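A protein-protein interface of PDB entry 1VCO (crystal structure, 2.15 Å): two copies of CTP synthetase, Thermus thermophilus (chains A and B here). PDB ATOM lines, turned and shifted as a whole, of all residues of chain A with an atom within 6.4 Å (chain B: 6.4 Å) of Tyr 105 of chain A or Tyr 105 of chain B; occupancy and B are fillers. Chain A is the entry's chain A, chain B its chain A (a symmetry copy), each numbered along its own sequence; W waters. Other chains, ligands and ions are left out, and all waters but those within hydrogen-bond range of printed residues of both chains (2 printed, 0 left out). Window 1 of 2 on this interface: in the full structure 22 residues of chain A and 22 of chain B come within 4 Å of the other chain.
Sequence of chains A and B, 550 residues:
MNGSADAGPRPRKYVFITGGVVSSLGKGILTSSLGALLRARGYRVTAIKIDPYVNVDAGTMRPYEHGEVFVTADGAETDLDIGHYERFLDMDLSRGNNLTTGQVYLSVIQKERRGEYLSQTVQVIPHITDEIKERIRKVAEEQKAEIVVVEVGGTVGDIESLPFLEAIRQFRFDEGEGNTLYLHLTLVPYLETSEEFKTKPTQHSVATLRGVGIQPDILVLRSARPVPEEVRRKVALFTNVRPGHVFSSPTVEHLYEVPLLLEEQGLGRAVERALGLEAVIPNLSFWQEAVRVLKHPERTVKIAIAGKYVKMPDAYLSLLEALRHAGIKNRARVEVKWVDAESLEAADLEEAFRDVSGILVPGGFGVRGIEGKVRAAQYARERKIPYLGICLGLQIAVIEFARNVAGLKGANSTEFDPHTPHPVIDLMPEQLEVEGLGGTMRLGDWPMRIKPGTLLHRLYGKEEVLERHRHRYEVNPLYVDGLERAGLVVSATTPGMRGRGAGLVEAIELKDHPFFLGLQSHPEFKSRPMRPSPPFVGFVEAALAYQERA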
ATOM      1  N   VAL A  54      -4.746 -14.610 -18.152  1.00  0.00           N
ATOM      2  CA  VAL A  54      -4.934 -15.206 -16.844  1.00  0.00           C
ATOM      3  C   VAL A  54      -3.840 -14.910 -15.820  1.00  0.00           C
ATOM      4  O   VAL A  54      -4.057 -15.081 -14.621  1.00  0.00           O
ATOM      5  CB  VAL A  54      -5.139 -16.734 -17.001  1.00  0.00           C
ATOM      6  CG1 VAL A  54      -5.415 -17.378 -15.657  1.00  0.00           C
ATOM      7  CG2 VAL A  54      -6.314 -16.992 -17.955  1.00  0.00           C
ATOM      8  N   THR A 100      -6.235  -7.656 -14.832  1.00  0.00           N
ATOM      9  CA  THR A 100      -6.157  -8.913 -15.582  1.00  0.00           C
ATOM     10  C   THR A 100      -7.247  -9.899 -15.188  1.00  0.00           C
ATOM     11  O   THR A 100      -7.906  -9.726 -14.164  1.00  0.00           O
ATOM     12  CB  THR A 100      -4.805  -9.608 -15.342  1.00  0.00           C
ATOM     13  OG1 THR A 100      -4.716  -9.988 -13.963  1.00  0.00           O
ATOM     14  CG2 THR A 100      -3.643  -8.664 -15.672  1.00  0.00           C
ATOM     15  N   THR A 101      -7.431 -10.937 -15.997  1.00  0.00           N
ATOM     16  CA  THR A 101      -8.418 -11.960 -15.691  1.00  0.00           C
ATOM     17  C   THR A 101      -8.012 -12.676 -14.389  1.00  0.00           C
ATOM     18  O   THR A 101      -8.841 -12.917 -13.522  1.00  0.00           O
ATOM     19  CB  THR A 101      -8.519 -13.000 -16.836  1.00  0.00           C
ATOM     20  OG1 THR A 101      -9.096 -12.380 -17.988  1.00  0.00           O
ATOM     21  CG2 THR A 101      -9.374 -14.194 -16.419  1.00  0.00           C
ATOM     22  N   GLY A 102      -6.732 -13.011 -14.258  1.00  0.00           N
ATOM     23  CA  GLY A 102      -6.262 -13.682 -13.053  1.00  0.00           C
ATOM     24  C   GLY A 102      -6.600 -12.923 -11.777  1.00  0.00           C
ATOM     25  O   GLY A 102      -7.073 -13.514 -10.804  1.00  0.00           O
ATOM     26  N   GLN A 103      -6.364 -11.613 -11.775  1.00  0.00           N
ATOM     27  CA  GLN A 103      -6.666 -10.782 -10.604  1.00  0.00           C
ATOM     28  C   GLN A 103      -8.140 -10.884 -10.234  1.00  0.00           C
ATOM     29  O   GLN A 103      -8.493 -11.190  -9.099  1.00  0.00           O
ATOM     30  CB  GLN A 103      -6.355  -9.309 -10.893  1.00  0.00           C
ATOM     31  CG  GLN A 103      -4.888  -8.945 -10.915  1.00  0.00           C
ATOM     32  CD  GLN A 103      -4.650  -7.547 -11.474  1.00  0.00           C
ATOM     33  OE1 GLN A 103      -5.563  -6.720 -11.524  1.00  0.00           O
ATOM     34  NE2 GLN A 103      -3.415  -7.278 -11.885  1.00  0.00           N
ATOM     35  N   VAL A 104      -8.993 -10.627 -11.220  1.00  0.00           N
ATOM     36  CA  VAL A 104     -10.439 -10.644 -11.039  1.00  0.00           C
ATOM     37  C   VAL A 104     -11.018 -11.975 -10.586  1.00  0.00           C
ATOM     38  O   VAL A 104     -11.795 -12.028  -9.631  1.00  0.00           O
ATOM     39  CB  VAL A 104     -11.139 -10.187 -12.340  1.00  0.00           C
ATOM     40  CG1 VAL A 104     -12.633 -10.442 -12.247  1.00  0.00           C
ATOM     41  CG2 VAL A 104     -10.864  -8.695 -12.560  1.00  0.00           C
ATOM     42  N   TYR A 105     -10.670 -13.056 -11.276  1.00  0.00           N
ATOM     43  CA  TYR A 105     -11.191 -14.341 -10.866  1.00  0.00           C
ATOM     44  C   TYR A 105     -10.603 -14.761  -9.510  1.00  0.00           C
ATOM     45  O   TYR A 105     -11.312 -15.318  -8.680  1.00  0.00           O
ATOM     46  CB  TYR A 105     -10.937 -15.406 -11.950  1.00  0.00           C
ATOM     47  CG  TYR A 105     -11.942 -15.358 -13.106  1.00  0.00           C
ATOM     48  CD1 TYR A 105     -11.962 -14.289 -14.002  1.00  0.00           C
ATOM     49  CD2 TYR A 105     -12.874 -16.375 -13.281  1.00  0.00           C
ATOM     50  CE1 TYR A 105     -12.894 -14.242 -15.056  1.00  0.00           C
ATOM     51  CE2 TYR A 105     -13.808 -16.341 -14.319  1.00  0.00           C
ATOM     52  CZ  TYR A 105     -13.812 -15.274 -15.203  1.00  0.00           C
ATOM     53  OH  TYR A 105     -14.719 -15.258 -16.235  1.00  0.00           O
ATOM     54  N   LEU A 106      -9.325 -14.472  -9.263  1.00  0.00           N
ATOM     55  CA  LEU A 106      -8.715 -14.855  -7.982  1.00  0.00           C
ATOM     56  C   LEU A 106      -9.383 -14.174  -6.775  1.00  0.00           C
ATOM     57  O   LEU A 106      -9.677 -14.840  -5.775  1.00  0.00           O
ATOM     58  CB  LEU A 106      -7.208 -14.550  -7.970  1.00  0.00           C
ATOM     59  CG  LEU A 106      -6.481 -15.020  -6.693  1.00  0.00           C
ATOM     60  CD1 LEU A 106      -6.657 -16.522  -6.537  1.00  0.00           C
ATOM     61  CD2 LEU A 106      -4.997 -14.656  -6.744  1.00  0.00           C
ATOM     62  N   SER A 107      -9.639 -12.870  -6.858  1.00  0.00           N
ATOM     63  CA  SER A 107     -10.270 -12.165  -5.730  1.00  0.00           C
ATOM     64  C   SER A 107     -11.671 -12.696  -5.467  1.00  0.00           C
ATOM     65  O   SER A 107     -12.041 -12.952  -4.322  1.00  0.00           O
ATOM     66  CB  SER A 107     -10.365 -10.652  -5.987  1.00  0.00           C
ATOM     67  OG  SER A 107      -9.092 -10.082  -6.215  1.00  0.00           O
ATOM     68  N   VAL A 108     -12.454 -12.854  -6.528  1.00  0.00           N
ATOM     69  CA  VAL A 108     -13.814 -13.348  -6.388  1.00  0.00           C
ATOM     70  C   VAL A 108     -13.809 -14.767  -5.836  1.00  0.00           C
ATOM     71  O   VAL A 108     -14.616 -15.106  -4.967  1.00  0.00           O
ATOM     72  CB  VAL A 108     -14.568 -13.320  -7.739  1.00  0.00           C
ATOM     73  CG1 VAL A 108     -15.900 -14.019  -7.613  1.00  0.00           C
ATOM     74  CG2 VAL A 108     -14.791 -11.878  -8.169  1.00  0.00           C
ATOM     75  N   ILE A 109     -12.897 -15.592  -6.333  1.00  0.00           N
ATOM     76  CA  ILE A 109     -12.812 -16.970  -5.878  1.00  0.00           C
ATOM     77  C   ILE A 109     -12.371 -17.043  -4.416  1.00  0.00           C
ATOM     78  O   ILE A 109     -12.984 -17.758  -3.622  1.00  0.00           O
ATOM     79  CB  ILE A 109     -11.844 -17.777  -6.751  1.00  0.00           C
ATOM     80  CG1 ILE A 109     -12.484 -18.033  -8.120  1.00  0.00           C
ATOM     81  CG2 ILE A 109     -11.500 -19.096  -6.063  1.00  0.00           C
ATOM     82  CD1 ILE A 109     -11.545 -18.673  -9.110  1.00  0.00           C
ATOM     83  N   GLN A 110     -11.321 -16.305  -4.066  1.00  0.00           N
ATOM     84  CA  GLN A 110     -10.845 -16.294  -2.683  1.00  0.00           C
ATOM     85  C   GLN A 110     -11.967 -15.766  -1.790  1.00  0.00           C
ATOM     86  O   GLN A 110     -12.156 -16.235  -0.670  1.00  0.00           O
ATOM     87  CB  GLN A 110      -9.593 -15.411  -2.532  1.00  0.00           C
ATOM     88  CG  GLN A 110      -8.373 -15.925  -3.295  1.00  0.00           C
ATOM     89  CD  GLN A 110      -7.149 -15.033  -3.146  1.00  0.00           C
ATOM     90  OE1 GLN A 110      -7.262 -13.811  -3.075  1.00  0.00           O
ATOM     91  NE2 GLN A 110      -5.969 -15.644  -3.117  1.00  0.00           N
ATOM     92  N   VAL A 124     -20.030 -15.408 -13.091  1.00  0.00           N
ATOM     93  CA  VAL A 124     -19.320 -14.417 -13.895  1.00  0.00           C
ATOM     94  C   VAL A 124     -20.154 -13.138 -13.845  1.00  0.00           C
ATOM     95  O   VAL A 124     -19.642 -12.053 -13.583  1.00  0.00           O
ATOM     96  CB  VAL A 124     -19.153 -14.924 -15.349  1.00  0.00           C
ATOM     97  CG1 VAL A 124     -18.654 -13.813 -16.250  1.00  0.00           C
ATOM     98  CG2 VAL A 124     -18.174 -16.085 -15.364  1.00  0.00           C
ATOM     99  N   ILE A 128     -18.229 -11.653 -11.102  1.00  0.00           N
ATOM    100  CA  ILE A 128     -16.955 -11.341 -11.736  1.00  0.00           C
ATOM    101  C   ILE A 128     -17.059  -9.924 -12.316  1.00  0.00           C
ATOM    102  O   ILE A 128     -16.148  -9.114 -12.158  1.00  0.00           O
ATOM    103  CB  ILE A 128     -16.610 -12.340 -12.870  1.00  0.00           C
ATOM    104  CG1 ILE A 128     -16.321 -13.729 -12.287  1.00  0.00           C
ATOM    105  CG2 ILE A 128     -15.404 -11.835 -13.650  1.00  0.00           C
ATOM    106  CD1 ILE A 128     -15.120 -13.770 -11.311  1.00  0.00           C
ATOM    107  N   GLU A 131     -16.665  -7.198  -9.646  1.00  0.00           N
ATOM    108  CA  GLU A 131     -15.263  -7.051  -9.259  1.00  0.00           C
ATOM    109  C   GLU A 131     -14.523  -6.152 -10.250  1.00  0.00           C
ATOM    110  O   GLU A 131     -13.787  -5.242  -9.850  1.00  0.00           O
ATOM    111  CB  GLU A 131     -14.592  -8.430  -9.191  1.00  0.00           C
ATOM    112  CG  GLU A 131     -13.117  -8.394  -8.830  1.00  0.00           C
ATOM    113  CD  GLU A 131     -12.858  -7.922  -7.402  1.00  0.00           C
ATOM    114  OE1 GLU A 131     -11.689  -7.626  -7.083  1.00  0.00           O
ATOM    115  OE2 GLU A 131     -13.810  -7.853  -6.597  1.00  0.00           O
ATOM    116  N   ILE A 132     -14.726  -6.400 -11.545  1.00  0.00           N
ATOM    117  CA  ILE A 132     -14.083  -5.611 -12.599  1.00  0.00           C
ATOM    118  C   ILE A 132     -14.452  -4.126 -12.494  1.00  0.00           C
ATOM    119  O   ILE A 132     -13.585  -3.256 -12.507  1.00  0.00           O
ATOM    120  CB  ILE A 132     -14.493  -6.117 -14.014  1.00  0.00           C
ATOM    121  CG1 ILE A 132     -13.944  -7.527 -14.244  1.00  0.00           C
ATOM    122  CG2 ILE A 132     -13.991  -5.145 -15.084  1.00  0.00           C
ATOM    123  CD1 ILE A 132     -14.601  -8.260 -15.420  1.00  0.00           C
ATOM    124  N   ILE A 159     -13.011 -15.119 -26.676  1.00  0.00           N
ATOM    125  CA  ILE A 159     -13.627 -15.541 -25.436  1.00  0.00           C
ATOM    126  C   ILE A 159     -13.142 -14.778 -24.204  1.00  0.00           C
ATOM    127  O   ILE A 159     -13.956 -14.275 -23.437  1.00  0.00           O
ATOM    128  CB  ILE A 159     -13.447 -17.079 -25.259  1.00  0.00           C
ATOM    129  CG1 ILE A 159     -14.408 -17.808 -26.213  1.00  0.00           C
ATOM    130  CG2 ILE A 159     -13.696 -17.504 -23.821  1.00  0.00           C
ATOM    131  CD1 ILE A 159     -14.283 -19.336 -26.189  1.00  0.00           C
ATOM    132  N   PRO A 163     -15.984 -11.172 -20.316  1.00  0.00           N
ATOM    133  CA  PRO A 163     -16.384 -10.665 -18.996  1.00  0.00           C
ATOM    134  C   PRO A 163     -16.122  -9.168 -18.866  1.00  0.00           C
ATOM    135  O   PRO A 163     -16.869  -8.448 -18.207  1.00  0.00           O
ATOM    136  CB  PRO A 163     -15.521 -11.477 -18.032  1.00  0.00           C
ATOM    137  CG  PRO A 163     -15.329 -12.782 -18.768  1.00  0.00           C
ATOM    138  CD  PRO A 163     -15.060 -12.316 -20.188  1.00  0.00           C
ATOM    139  N   PHE A 164     -15.057  -8.700 -19.502  1.00  0.00           N
ATOM    140  CA  PHE A 164     -14.704  -7.289 -19.436  1.00  0.00           C
ATOM    141  C   PHE A 164     -15.597  -6.413 -20.311  1.00  0.00           C
ATOM    142  O   PHE A 164     -15.931  -5.294 -19.932  1.00  0.00           O
ATOM    143  CB  PHE A 164     -13.233  -7.109 -19.807  1.00  0.00           C
ATOM    144  CG  PHE A 164     -12.288  -7.728 -18.809  1.00  0.00           C
ATOM    145  CD1 PHE A 164     -12.113  -7.154 -17.553  1.00  0.00           C
ATOM    146  CD2 PHE A 164     -11.622  -8.916 -19.098  1.00  0.00           C
ATOM    147  CE1 PHE A 164     -11.293  -7.758 -16.598  1.00  0.00           C
ATOM    148  CE2 PHE A 164     -10.798  -9.531 -18.150  1.00  0.00           C
ATOM    149  CZ  PHE A 164     -10.635  -8.951 -16.898  1.00  0.00           C
ATOM    150  N   VAL B  54     -18.892 -19.881 -10.378  1.00  0.00           N
ATOM    151  CA  VAL B  54     -17.579 -19.580  -9.840  1.00  0.00           C
ATOM    152  C   VAL B  54     -17.240 -20.253  -8.511  1.00  0.00           C
ATOM    153  O   VAL B  54     -16.068 -20.332  -8.144  1.00  0.00           O
ATOM    154  CB  VAL B  54     -17.407 -18.043  -9.737  1.00  0.00           C
ATOM    155  CG1 VAL B  54     -16.015 -17.693  -9.250  1.00  0.00           C
ATOM    156  CG2 VAL B  54     -17.653 -17.412 -11.115  1.00  0.00           C
ATOM    157  N   THR B 100     -16.269 -27.133 -11.836  1.00  0.00           N
ATOM    158  CA  THR B 100     -16.783 -25.761 -11.804  1.00  0.00           C
ATOM    159  C   THR B 100     -15.792 -24.749 -12.359  1.00  0.00           C
ATOM    160  O   THR B 100     -14.614 -25.058 -12.531  1.00  0.00           O
ATOM    161  CB  THR B 100     -17.111 -25.334 -10.362  1.00  0.00           C
ATOM    162  OG1 THR B 100     -15.897 -25.297  -9.602  1.00  0.00           O
ATOM    163  CG2 THR B 100     -18.075 -26.331  -9.707  1.00  0.00           C
ATOM    164  N   THR B 101     -16.266 -23.538 -12.631  1.00  0.00           N
ATOM    165  CA  THR B 101     -15.394 -22.484 -13.125  1.00  0.00           C
ATOM    166  C   THR B 101     -14.348 -22.150 -12.045  1.00  0.00           C
ATOM    167  O   THR B 101     -13.170 -22.000 -12.339  1.00  0.00           O
ATOM    168  CB  THR B 101     -16.200 -21.207 -13.470  1.00  0.00           C
ATOM    169  OG1 THR B 101     -17.022 -21.459 -14.613  1.00  0.00           O
ATOM    170  CG2 THR B 101     -15.269 -20.032 -13.761  1.00  0.00           C
ATOM    171  N   GLY B 102     -14.787 -22.036 -10.795  1.00  0.00           N
ATOM    172  CA  GLY B 102     -13.863 -21.731  -9.711  1.00  0.00           C
ATOM    173  C   GLY B 102     -12.697 -22.707  -9.629  1.00  0.00           C
ATOM    174  O   GLY B 102     -11.544 -22.295  -9.485  1.00  0.00           O
ATOM    175  N   GLN B 103     -12.989 -24.003  -9.722  1.00  0.00           N
ATOM    176  CA  GLN B 103     -11.941 -25.030  -9.670  1.00  0.00           C
ATOM    177  C   GLN B 103     -10.914 -24.810 -10.772  1.00  0.00           C
ATOM    178  O   GLN B 103      -9.716 -24.727 -10.520  1.00  0.00           O
ATOM    179  CB  GLN B 103     -12.545 -26.426  -9.861  1.00  0.00           C
ATOM    180  CG  GLN B 103     -13.303 -26.976  -8.674  1.00  0.00           C
ATOM    181  CD  GLN B 103     -14.097 -28.228  -9.028  1.00  0.00           C
ATOM    182  OE1 GLN B 103     -13.828 -28.886 -10.036  1.00  0.00           O
ATOM    183  NE2 GLN B 103     -15.072 -28.566  -8.190  1.00  0.00           N
ATOM    184  N   VAL B 104     -11.410 -24.713 -12.001  1.00  0.00           N
ATOM    185  CA  VAL B 104     -10.573 -24.536 -13.181  1.00  0.00           C
ATOM    186  C   VAL B 104      -9.721 -23.277 -13.185  1.00  0.00           C
ATOM    187  O   VAL B 104      -8.516 -23.337 -13.438  1.00  0.00           O
ATOM    188  CB  VAL B 104     -11.444 -24.580 -14.458  1.00  0.00           C
ATOM    189  CG1 VAL B 104     -10.627 -24.148 -15.662  1.00  0.00           C
ATOM    190  CG2 VAL B 104     -11.973 -26.006 -14.655  1.00  0.00           C
ATOM    191  N   TYR B 105     -10.334 -22.126 -12.932  1.00  0.00           N
ATOM    192  CA  TYR B 105      -9.553 -20.909 -12.915  1.00  0.00           C
ATOM    193  C   TYR B 105      -8.587 -20.898 -11.720  1.00  0.00           C
ATOM    194  O   TYR B 105      -7.453 -20.453 -11.852  1.00  0.00           O
ATOM    195  CB  TYR B 105     -10.469 -19.670 -12.918  1.00  0.00           C
ATOM    196  CG  TYR B 105     -11.014 -19.312 -14.304  1.00  0.00           C
ATOM    197  CD1 TYR B 105     -11.935 -20.133 -14.954  1.00  0.00           C
ATOM    198  CD2 TYR B 105     -10.588 -18.162 -14.960  1.00  0.00           C
ATOM    199  CE1 TYR B 105     -12.424 -19.807 -16.233  1.00  0.00           C
ATOM    200  CE2 TYR B 105     -11.060 -17.826 -16.231  1.00  0.00           C
ATOM    201  CZ  TYR B 105     -11.979 -18.651 -16.860  1.00  0.00           C
ATOM    202  OH  TYR B 105     -12.456 -18.304 -18.101  1.00  0.00           O
ATOM    203  N   LEU B 106      -9.011 -21.411 -10.565  1.00  0.00           N
ATOM    204  CA  LEU B 106      -8.126 -21.420  -9.392  1.00  0.00           C
ATOM    205  C   LEU B 106      -6.855 -22.260  -9.609  1.00  0.00           C
ATOM    206  O   LEU B 106      -5.752 -21.807  -9.281  1.00  0.00           O
ATOM    207  CB  LEU B 106      -8.864 -21.927  -8.142  1.00  0.00           C
ATOM    208  CG  LEU B 106      -8.025 -21.869  -6.848  1.00  0.00           C
ATOM    209  CD1 LEU B 106      -7.597 -20.434  -6.590  1.00  0.00           C
ATOM    210  CD2 LEU B 106      -8.816 -22.416  -5.659  1.00  0.00           C
ATOM    211  N   SER B 107      -6.989 -23.462 -10.167  1.00  0.00           N
ATOM    212  CA  SER B 107      -5.808 -24.311 -10.392  1.00  0.00           C
ATOM    213  C   SER B 107      -4.848 -23.665 -11.378  1.00  0.00           C
ATOM    214  O   SER B 107      -3.641 -23.629 -11.148  1.00  0.00           O
ATOM    215  CB  SER B 107      -6.199 -25.696 -10.932  1.00  0.00           C
ATOM    216  OG  SER B 107      -7.074 -26.371 -10.051  1.00  0.00           O
ATOM    217  N   VAL B 108      -5.385 -23.160 -12.484  1.00  0.00           N
ATOM    218  CA  VAL B 108      -4.556 -22.526 -13.497  1.00  0.00           C
ATOM    219  C   VAL B 108      -3.879 -21.286 -12.929  1.00  0.00           C
ATOM    220  O   VAL B 108      -2.696 -21.046 -13.179  1.00  0.00           O
ATOM    221  CB  VAL B 108      -5.386 -22.138 -14.744  1.00  0.00           C
ATOM    222  CG1 VAL B 108      -4.554 -21.307 -15.692  1.00  0.00           C
ATOM    223  CG2 VAL B 108      -5.858 -23.398 -15.455  1.00  0.00           C
ATOM    224  N   ILE B 109      -4.625 -20.505 -12.158  1.00  0.00           N
ATOM    225  CA  ILE B 109      -4.075 -19.294 -11.573  1.00  0.00           C
ATOM    226  C   ILE B 109      -2.997 -19.620 -10.540  1.00  0.00           C
ATOM    227  O   ILE B 109      -1.917 -19.027 -10.568  1.00  0.00           O
ATOM    228  CB  ILE B 109      -5.178 -18.451 -10.920  1.00  0.00           C
ATOM    229  CG1 ILE B 109      -6.037 -17.802 -12.011  1.00  0.00           C
ATOM    230  CG2 ILE B 109      -4.554 -17.386 -10.021  1.00  0.00           C
ATOM    231  CD1 ILE B 109      -7.251 -17.089 -11.473  1.00  0.00           C
ATOM    232  N   GLN B 110      -3.286 -20.558  -9.642  1.00  0.00           N
ATOM    233  CA  GLN B 110      -2.305 -20.952  -8.631  1.00  0.00           C
ATOM    234  C   GLN B 110      -1.073 -21.509  -9.345  1.00  0.00           C
ATOM    235  O   GLN B 110       0.057 -21.287  -8.920  1.00  0.00           O
ATOM    236  CB  GLN B 110      -2.882 -22.012  -7.676  1.00  0.00           C
ATOM    237  CG  GLN B 110      -4.048 -21.512  -6.825  1.00  0.00           C
ATOM    238  CD  GLN B 110      -4.616 -22.576  -5.896  1.00  0.00           C
ATOM    239  OE1 GLN B 110      -4.672 -23.754  -6.244  1.00  0.00           O
ATOM    240  NE2 GLN B 110      -5.058 -22.158  -4.715  1.00  0.00           N
ATOM    241  N   VAL B 124      -7.204 -18.137 -21.342  1.00  0.00           N
ATOM    242  CA  VAL B 124      -8.377 -19.007 -21.297  1.00  0.00           C
ATOM    243  C   VAL B 124      -8.120 -20.135 -22.296  1.00  0.00           C
ATOM    244  O   VAL B 124      -8.283 -21.311 -21.985  1.00  0.00           O
ATOM    245  CB  VAL B 124      -9.652 -18.209 -21.663  1.00  0.00           C
ATOM    246  CG1 VAL B 124     -10.827 -19.142 -21.872  1.00  0.00           C
ATOM    247  CG2 VAL B 124      -9.962 -17.224 -20.549  1.00  0.00           C
ATOM    248  N   ILE B 128      -6.837 -22.463 -19.772  1.00  0.00           N
ATOM    249  CA  ILE B 128      -8.030 -22.795 -19.006  1.00  0.00           C
ATOM    250  C   ILE B 128      -8.685 -24.013 -19.672  1.00  0.00           C
ATOM    251  O   ILE B 128      -9.088 -24.957 -18.995  1.00  0.00           O
ATOM    252  CB  ILE B 128      -9.042 -21.621 -18.966  1.00  0.00           C
ATOM    253  CG1 ILE B 128      -8.475 -20.458 -18.144  1.00  0.00           C
ATOM    254  CG2 ILE B 128     -10.358 -22.098 -18.366  1.00  0.00           C
ATOM    255  CD1 ILE B 128      -8.180 -20.809 -16.666  1.00  0.00           C
ATOM    256  N   GLU B 131      -6.921 -27.306 -18.800  1.00  0.00           N
ATOM    257  CA  GLU B 131      -7.261 -27.732 -17.443  1.00  0.00           C
ATOM    258  C   GLU B 131      -8.598 -28.474 -17.432  1.00  0.00           C
ATOM    259  O   GLU B 131      -8.721 -29.545 -16.826  1.00  0.00           O
ATOM    260  CB  GLU B 131      -7.323 -26.513 -16.513  1.00  0.00           C
ATOM    261  CG  GLU B 131      -7.705 -26.836 -15.078  1.00  0.00           C
ATOM    262  CD  GLU B 131      -6.647 -27.654 -14.344  1.00  0.00           C
ATOM    263  OE1 GLU B 131      -6.958 -28.176 -13.254  1.00  0.00           O
ATOM    264  OE2 GLU B 131      -5.508 -27.772 -14.842  1.00  0.00           O
ATOM    265  N   ILE B 132      -9.598 -27.910 -18.112  1.00  0.00           N
ATOM    266  CA  ILE B 132     -10.929 -28.518 -18.187  1.00  0.00           C
ATOM    267  C   ILE B 132     -10.871 -29.921 -18.803  1.00  0.00           C
ATOM    268  O   ILE B 132     -11.410 -30.878 -18.252  1.00  0.00           O
ATOM    269  CB  ILE B 132     -11.900 -27.649 -19.039  1.00  0.00           C
ATOM    270  CG1 ILE B 132     -12.162 -26.315 -18.337  1.00  0.00           C
ATOM    271  CG2 ILE B 132     -13.204 -28.411 -19.286  1.00  0.00           C
ATOM    272  CD1 ILE B 132     -12.777 -25.248 -19.250  1.00  0.00           C
ATOM    273  N   ILE B 159     -22.384 -16.283 -21.152  1.00  0.00           N
ATOM    274  CA  ILE B 159     -20.954 -16.075 -21.058  1.00  0.00           C
ATOM    275  C   ILE B 159     -20.213 -17.160 -20.277  1.00  0.00           C
ATOM    276  O   ILE B 159     -19.233 -17.707 -20.772  1.00  0.00           O
ATOM    277  CB  ILE B 159     -20.670 -14.659 -20.471  1.00  0.00           C
ATOM    278  CG1 ILE B 159     -20.950 -13.603 -21.555  1.00  0.00           C
ATOM    279  CG2 ILE B 159     -19.239 -14.544 -19.970  1.00  0.00           C
ATOM    280  CD1 ILE B 159     -20.774 -12.155 -21.085  1.00  0.00           C
ATOM    281  N   PRO B 163     -15.994 -21.128 -21.903  1.00  0.00           N
ATOM    282  CA  PRO B 163     -14.725 -21.863 -21.798  1.00  0.00           C
ATOM    283  C   PRO B 163     -14.943 -23.372 -21.857  1.00  0.00           C
ATOM    284  O   PRO B 163     -14.119 -24.111 -22.389  1.00  0.00           O
ATOM    285  CB  PRO B 163     -14.176 -21.421 -20.443  1.00  0.00           C
ATOM    286  CG  PRO B 163     -14.726 -20.023 -20.295  1.00  0.00           C
ATOM    287  CD  PRO B 163     -16.155 -20.184 -20.780  1.00  0.00           C
ATOM    288  N   PHE B 164     -16.063 -23.825 -21.309  1.00  0.00           N
ATOM    289  CA  PHE B 164     -16.368 -25.249 -21.297  1.00  0.00           C
ATOM    290  C   PHE B 164     -16.834 -25.767 -22.654  1.00  0.00           C
ATOM    291  O   PHE B 164     -16.503 -26.886 -23.039  1.00  0.00           O
ATOM    292  CB  PHE B 164     -17.406 -25.543 -20.215  1.00  0.00           C
ATOM    293  CG  PHE B 164     -16.892 -25.307 -18.817  1.00  0.00           C
ATOM    294  CD1 PHE B 164     -15.958 -26.172 -18.254  1.00  0.00           C
ATOM    295  CD2 PHE B 164     -17.290 -24.189 -18.090  1.00  0.00           C
ATOM    296  CE1 PHE B 164     -15.425 -25.923 -16.988  1.00  0.00           C
ATOM    297  CE2 PHE B 164     -16.763 -23.929 -16.820  1.00  0.00           C
ATOM    298  CZ  PHE B 164     -15.829 -24.797 -16.270  1.00  0.00           C
HETATM  299  O   HOH W   1     -12.515 -15.697 -18.772  1.00  0.00           O
HETATM  300  O   HOH W   2     -15.640 -17.607 -17.173  1.00  0.00           O
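Hydrophobic or aromatic side chains of chain A within 4 Å of the printed part of chain B: Val 54, Tyr 105, Ile 109, Val 124 and Ile 159. Among the printed residues, 9 pairs touch across the chains. Among the printed residues, no Asp or Glu carboxylate lies within 4 Å of a Lys or Arg side-chain nitrogen of the other chain.
Val 54 of chain A touches Ile 109 of chain B, and with the chains exchanged Ile 109 of chain A touches Val 54 of chain B. Val 54 of chain A touches Val 124 of chain B, and with the chains exchanged Val 124 of chain A touches Val 54 of chain B. Gly 102 of chain A touches Ile 109 of chain B, and with the chains exchanged Ile 109 of chain A touches Gly 102 of chain B. Tyr 105 of chain A touches its own counterpart, Tyr 105 of chain B. Positions printed for both chains: 54, 100, 101, 102, 103, 104, 105, 106, 107, 108, 109, 110, 124, 128, 131, 132, 159, 163 and 164.
The backbone carbonyl oxygen of Val 54 of chain A sits close to the backbone NH of Gly 102 of chain A, at 3.4 Å. O of Val 54 of chain B lies close to N of Gly 102 of chain B.
Ile 109 of chain B touches Val 54 of chain A. Val 54 of chain A touches Val 124 of chain B. Ile 109 of chain B touches Gly 102 of chain A. Tyr 105 of chain A touches Tyr 105 of chain B. CG1 of Val 54 of chain B touches CG1 of Ile 109 of chain A, 3.7 Å away. Ile 109 of chain A touches Gly 102 of chain B. Val 124 of chain A touches Val 54 of chain B. CG2 of Ile 159 of chain B touches CG1 of Val 124 of chain A (3.8 Å). CG2 of Ile 159 of chain A touches CG1 of Val 124 of chain B, at 3.8 Å.
Water W2 bridges the side-chain hydroxyl of Tyr 105 of chain A and the side-chain hydroxyl of Tyr 105 of chain B. Water W1 bridges the side-chain hydroxyl (OH) of Tyr 105 of chain B (2.7 Å) and the side-chain hydroxyl (OH) of Tyr 105 of chain A (3.4 Å).
Of the printed residues of chain A, Tyr 105 of chain B touches Tyr 105 (3.4 Å). Of the printed residues of chain B, Ile 109 of chain A touches Val 54 (3.7 Å) and Gly 102 (3.6 Å). Printed residues of chain A within 4 Å of Val 54 of chain B: Ile 109 and Val 124. Of the printed residues of chain B, Ile 159 of chain A touches Val 124 (3.8 Å). Printed residues of chain A within 4 Å of Ile 109 of chain B: Val 54 (3.7 Å) and Gly 102 (3.6 Å). The nearest printed residue of chain B that does not touch Tyr 105 of chain A is Thr 101 of chain B (4.01 Å).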
